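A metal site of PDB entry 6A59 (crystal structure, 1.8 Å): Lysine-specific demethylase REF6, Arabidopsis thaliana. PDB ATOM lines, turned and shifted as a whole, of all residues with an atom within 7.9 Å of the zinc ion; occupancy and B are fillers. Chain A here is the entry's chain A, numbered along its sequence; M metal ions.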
ATOM      1  N   GLN A  24       8.511 -17.653 -12.650  1.00  0.00           N
ATOM      2  CA  GLN A  24       8.728 -16.316 -12.075  1.00  0.00           C
ATOM      3  C   GLN A  24      10.088 -16.237 -11.371  1.00  0.00           C
ATOM      4  O   GLN A  24      10.519 -17.222 -10.755  1.00  0.00           O
ATOM      5  CB  GLN A  24       7.615 -15.973 -11.078  1.00  0.00           C
ATOM      6  CG  GLN A  24       6.237 -15.753 -11.696  1.00  0.00           C
ATOM      7  CD  GLN A  24       5.449 -17.028 -11.988  1.00  0.00           C
ATOM      8  OE1 GLN A  24       5.731 -18.099 -11.440  1.00  0.00           O
ATOM      9  NE2 GLN A  24       4.455 -16.912 -12.873  1.00  0.00           N
ATOM     10  N   CYS A  25      10.761 -15.094 -11.466  1.00  0.00           N
ATOM     11  CA  CYS A  25      12.008 -14.847 -10.733  1.00  0.00           C
ATOM     12  C   CYS A  25      11.713 -14.540  -9.265  1.00  0.00           C
ATOM     13  O   CYS A  25      10.817 -13.737  -8.963  1.00  0.00           O
ATOM     14  CB  CYS A  25      12.800 -13.696 -11.332  1.00  0.00           C
ATOM     15  SG  CYS A  25      14.354 -13.340 -10.454  1.00  0.00           S
ATOM     16  N   ASN A  26      12.490 -15.145  -8.367  1.00  0.00           N
ATOM     17  CA  ASN A  26      12.315 -14.990  -6.915  1.00  0.00           C
ATOM     18  C   ASN A  26      13.240 -13.967  -6.260  1.00  0.00           C
ATOM     19  O   ASN A  26      13.238 -13.839  -5.031  1.00  0.00           O
ATOM     20  CB  ASN A  26      12.431 -16.356  -6.207  1.00  0.00           C
ATOM     21  CG  ASN A  26      13.839 -16.941  -6.242  1.00  0.00           C
ATOM     22  OD1 ASN A  26      14.689 -16.520  -7.031  1.00  0.00           O
ATOM     23  ND2 ASN A  26      14.086 -17.922  -5.379  1.00  0.00           N
ATOM     24  N   MET A  27      14.028 -13.234  -7.056  1.00  0.00           N
ATOM     25  CA  MET A  27      14.899 -12.179  -6.530  1.00  0.00           C
ATOM     26  C   MET A  27      14.052 -11.033  -6.005  1.00  0.00           C
ATOM     27  O   MET A  27      13.006 -10.715  -6.566  1.00  0.00           O
ATOM     28  CB  MET A  27      15.857 -11.665  -7.605  1.00  0.00           C
ATOM     29  CG  MET A  27      16.914 -12.672  -8.056  1.00  0.00           C
ATOM     30  SD  MET A  27      18.230 -12.925  -6.842  1.00  0.00           S
ATOM     31  CE  MET A  27      17.707 -14.468  -6.086  1.00  0.00           C
ATOM     32  N   GLU A  28      14.517 -10.418  -4.912  1.00  0.00           N
ATOM     33  CA  GLU A  28      13.761  -9.353  -4.244  1.00  0.00           C
ATOM     34  C   GLU A  28      13.521  -8.182  -5.196  1.00  0.00           C
ATOM     35  O   GLU A  28      14.466  -7.664  -5.801  1.00  0.00           O
ATOM     36  CB  GLU A  28      14.509  -8.885  -2.980  1.00  0.00           C
ATOM     37  CG  GLU A  28      13.761  -7.862  -2.117  1.00  0.00           C
ATOM     38  CD  GLU A  28      12.403  -8.348  -1.644  1.00  0.00           C
ATOM     39  OE1 GLU A  28      12.249  -9.551  -1.347  1.00  0.00           O
ATOM     40  OE2 GLU A  28      11.465  -7.512  -1.560  1.00  0.00           O
ATOM     41  N   GLY A  29      12.255  -7.815  -5.370  1.00  0.00           N
ATOM     42  CA  GLY A  29      11.868  -6.710  -6.247  1.00  0.00           C
ATOM     43  C   GLY A  29      11.648  -7.059  -7.715  1.00  0.00           C
ATOM     44  O   GLY A  29      11.091  -6.244  -8.452  1.00  0.00           O
ATOM     45  N   CYS A  30      12.072  -8.250  -8.155  1.00  0.00           N
ATOM     46  CA  CYS A  30      11.983  -8.613  -9.565  1.00  0.00           C
ATOM     47  C   CYS A  30      10.566  -9.033  -9.944  1.00  0.00           C
ATOM     48  O   CYS A  30       9.903  -9.756  -9.193  1.00  0.00           O
ATOM     49  CB  CYS A  30      12.939  -9.761  -9.915  1.00  0.00           C
ATOM     50  SG  CYS A  30      13.181  -9.938 -11.694  1.00  0.00           S
ATOM     51  N   THR A  31      10.111  -8.570 -11.104  1.00  0.00           N
ATOM     52  CA  THR A  31       8.779  -8.884 -11.607  1.00  0.00           C
ATOM     53  C   THR A  31       8.828  -9.640 -12.945  1.00  0.00           C
ATOM     54  O   THR A  31       7.800  -9.761 -13.619  1.00  0.00           O
ATOM     55  CB  THR A  31       7.925  -7.608 -11.746  1.00  0.00           C
ATOM     56  OG1 THR A  31       8.549  -6.718 -12.684  1.00  0.00           O
ATOM     57  CG2 THR A  31       7.779  -6.914 -10.393  1.00  0.00           C
ATOM     58  N   MET A  32       9.996 -10.161 -13.311  1.00  0.00           N
ATOM     59  CA  MET A  32      10.159 -10.862 -14.580  1.00  0.00           C
ATOM     60  C   MET A  32       9.727 -12.322 -14.488  1.00  0.00           C
ATOM     61  O   MET A  32       9.827 -12.941 -13.411  1.00  0.00           O
ATOM     62  CB  MET A  32      11.600 -10.787 -15.071  1.00  0.00           C
ATOM     63  CG  MET A  32      12.072  -9.364 -15.282  1.00  0.00           C
ATOM     64  SD  MET A  32      13.650  -9.279 -16.129  1.00  0.00           S
ATOM     65  CE  MET A  32      14.175  -7.637 -15.669  1.00  0.00           C
ATOM     66  N   SER A  33       9.243 -12.847 -15.606  1.00  0.00           N
ATOM     67  CA  SER A  33       8.870 -14.261 -15.737  1.00  0.00           C
ATOM     68  C   SER A  33       9.361 -14.783 -17.085  1.00  0.00           C
ATOM     69  O   SER A  33       9.656 -14.009 -17.984  1.00  0.00           O
ATOM     70  CB  SER A  33       7.359 -14.426 -15.616  1.00  0.00           C
ATOM     71  OG  SER A  33       6.685 -13.755 -16.653  1.00  0.00           O
ATOM     72  N   PHE A  34       9.434 -16.114 -17.193  1.00  0.00           N
ATOM     73  CA  PHE A  34      10.105 -16.785 -18.302  1.00  0.00           C
ATOM     74  C   PHE A  34       9.344 -18.022 -18.781  1.00  0.00           C
ATOM     75  O   PHE A  34       8.603 -18.633 -18.011  1.00  0.00           O
ATOM     76  CB  PHE A  34      11.543 -17.149 -17.892  1.00  0.00           C
ATOM     77  CG  PHE A  34      12.356 -15.953 -17.527  1.00  0.00           C
ATOM     78  CD1 PHE A  34      12.989 -15.216 -18.518  1.00  0.00           C
ATOM     79  CD2 PHE A  34      12.415 -15.506 -16.211  1.00  0.00           C
ATOM     80  CE1 PHE A  34      13.702 -14.086 -18.209  1.00  0.00           C
ATOM     81  CE2 PHE A  34      13.127 -14.360 -15.889  1.00  0.00           C
ATOM     82  CZ  PHE A  34      13.774 -13.650 -16.895  1.00  0.00           C
ATOM     83  N   LEU A  40      14.966 -19.009 -16.971  1.00  0.00           N
ATOM     84  CA  LEU A  40      15.019 -18.553 -15.562  1.00  0.00           C
ATOM     85  C   LEU A  40      16.408 -18.748 -14.970  1.00  0.00           C
ATOM     86  O   LEU A  40      16.911 -17.880 -14.257  1.00  0.00           O
ATOM     87  CB  LEU A  40      13.968 -19.281 -14.706  1.00  0.00           C
ATOM     88  CG  LEU A  40      13.950 -18.965 -13.208  1.00  0.00           C
ATOM     89  CD1 LEU A  40      13.696 -17.479 -12.959  1.00  0.00           C
ATOM     90  CD2 LEU A  40      12.915 -19.810 -12.476  1.00  0.00           C
ATOM     91  N   HIS A  43      18.652 -16.206 -16.448  1.00  0.00           N
ATOM     92  CA  HIS A  43      18.306 -14.957 -15.753  1.00  0.00           C
ATOM     93  C   HIS A  43      18.982 -14.827 -14.392  1.00  0.00           C
ATOM     94  O   HIS A  43      19.500 -13.769 -14.049  1.00  0.00           O
ATOM     95  CB  HIS A  43      16.798 -14.849 -15.575  1.00  0.00           C
ATOM     96  CG  HIS A  43      16.361 -13.541 -14.998  1.00  0.00           C
ATOM     97  ND1 HIS A  43      16.621 -12.350 -15.629  1.00  0.00           N
ATOM     98  CD2 HIS A  43      15.683 -13.238 -13.873  1.00  0.00           C
ATOM     99  CE1 HIS A  43      16.115 -11.363 -14.913  1.00  0.00           C
ATOM    100  NE2 HIS A  43      15.546 -11.874 -13.835  1.00  0.00           N
ATOM    101  N   LYS A  44      18.988 -15.920 -13.621  1.00  0.00           N
ATOM    102  CA  LYS A  44      19.677 -15.964 -12.320  1.00  0.00           C
ATOM    103  C   LYS A  44      21.215 -15.806 -12.416  1.00  0.00           C
ATOM    104  O   LYS A  44      21.853 -15.384 -11.453  1.00  0.00           O
ATOM    105  CB  LYS A  44      19.305 -17.224 -11.548  1.00  0.00           C
ATOM    106  CG  LYS A  44      17.891 -17.211 -11.019  1.00  0.00           C
ATOM    107  CD  LYS A  44      17.493 -18.557 -10.438  1.00  0.00           C
ATOM    108  CE  LYS A  44      16.353 -18.433  -9.440  1.00  0.00           C
ATOM    109  NZ  LYS A  44      16.777 -17.765  -8.171  1.00  0.00           N
ATOM    110  N   ASN A  46      22.377 -13.589 -14.319  1.00  0.00           N
ATOM    111  CA  ASN A  46      22.442 -12.187 -14.752  1.00  0.00           C
ATOM    112  C   ASN A  46      22.793 -11.989 -16.235  1.00  0.00           C
ATOM    113  O   ASN A  46      23.520 -11.052 -16.589  1.00  0.00           O
ATOM    114  CB  ASN A  46      23.378 -11.372 -13.838  1.00  0.00           C
ATOM    115  CG  ASN A  46      22.983 -11.451 -12.371  1.00  0.00           C
ATOM    116  OD1 ASN A  46      23.829 -11.658 -11.503  1.00  0.00           O
ATOM    117  ND2 ASN A  46      21.708 -11.262 -12.082  1.00  0.00           N
ATOM    118  N   HIS A  60      21.975  -8.601 -10.146  1.00  0.00           N
ATOM    119  CA  HIS A  60      20.609  -8.506 -10.655  1.00  0.00           C
ATOM    120  C   HIS A  60      20.164  -7.049 -10.823  1.00  0.00           C
ATOM    121  O   HIS A  60      19.410  -6.754 -11.751  1.00  0.00           O
ATOM    122  CB  HIS A  60      19.656  -9.295  -9.754  1.00  0.00           C
ATOM    123  CG  HIS A  60      18.219  -9.171 -10.151  1.00  0.00           C
ATOM    124  ND1 HIS A  60      17.349  -8.307  -9.527  1.00  0.00           N
ATOM    125  CD2 HIS A  60      17.507  -9.796 -11.121  1.00  0.00           C
ATOM    126  CE1 HIS A  60      16.167  -8.392 -10.090  1.00  0.00           C
ATOM    127  NE2 HIS A  60      16.231  -9.293 -11.059  1.00  0.00           N
ATOM    128  N   LEU A  63      21.467  -5.925 -14.146  1.00  0.00           N
ATOM    129  CA  LEU A  63      20.691  -6.599 -15.187  1.00  0.00           C
ATOM    130  C   LEU A  63      19.373  -5.876 -15.474  1.00  0.00           C
ATOM    131  O   LEU A  63      19.032  -5.647 -16.635  1.00  0.00           O
ATOM    132  CB  LEU A  63      20.410  -8.044 -14.784  1.00  0.00           C
ATOM    133  CG  LEU A  63      19.616  -8.897 -15.778  1.00  0.00           C
ATOM    134  CD1 LEU A  63      20.463  -9.202 -17.005  1.00  0.00           C
ATOM    135  CD2 LEU A  63      19.154 -10.162 -15.098  1.00  0.00           C
ATOM    136  N   VAL A  64      18.625  -5.558 -14.417  1.00  0.00           N
ATOM    137  CA  VAL A  64      17.307  -4.918 -14.552  1.00  0.00           C
ATOM    138  C   VAL A  64      17.443  -3.511 -15.150  1.00  0.00           C
ATOM    139  O   VAL A  64      16.644  -3.123 -16.020  1.00  0.00           O
ATOM    140  CB  VAL A  64      16.547  -4.857 -13.199  1.00  0.00           C
ATOM    141  CG1 VAL A  64      15.273  -4.028 -13.286  1.00  0.00           C
ATOM    142  CG2 VAL A  64      16.218  -6.269 -12.732  1.00  0.00           C
HETATM  143 ZN    ZN M   1      14.854 -11.422 -11.625  1.00  0.00          ZN
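The zinc ion is bound by SG of Cys 30 (2.2 Å), SG of Cys 25 (2.3 Å), NE2 of His 43 (2.4 Å) and NE2 of His 60 (2.6 Å).
The zinc ion has four donor atoms within binding distance.
ND2 of Asn 46 lies close to N of His 60 (3.3 Å).
SG of Cys 25 sits close to N of Met 27 (3.4 Å).
The side-chain sulfur (SG) of Cys 30 lies close to the backbone NH (N) of Met 32, 3.6 Å away.
N of Cys 25 lies within hydrogen-bond range of O of Met 32, at 3.0 Å.
Along chain A the residues within 4 Å of the zinc ion span positions 25 to 60.
The nearest printed residue that does not touch the zinc ion is Met 27 (4.2 Å).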
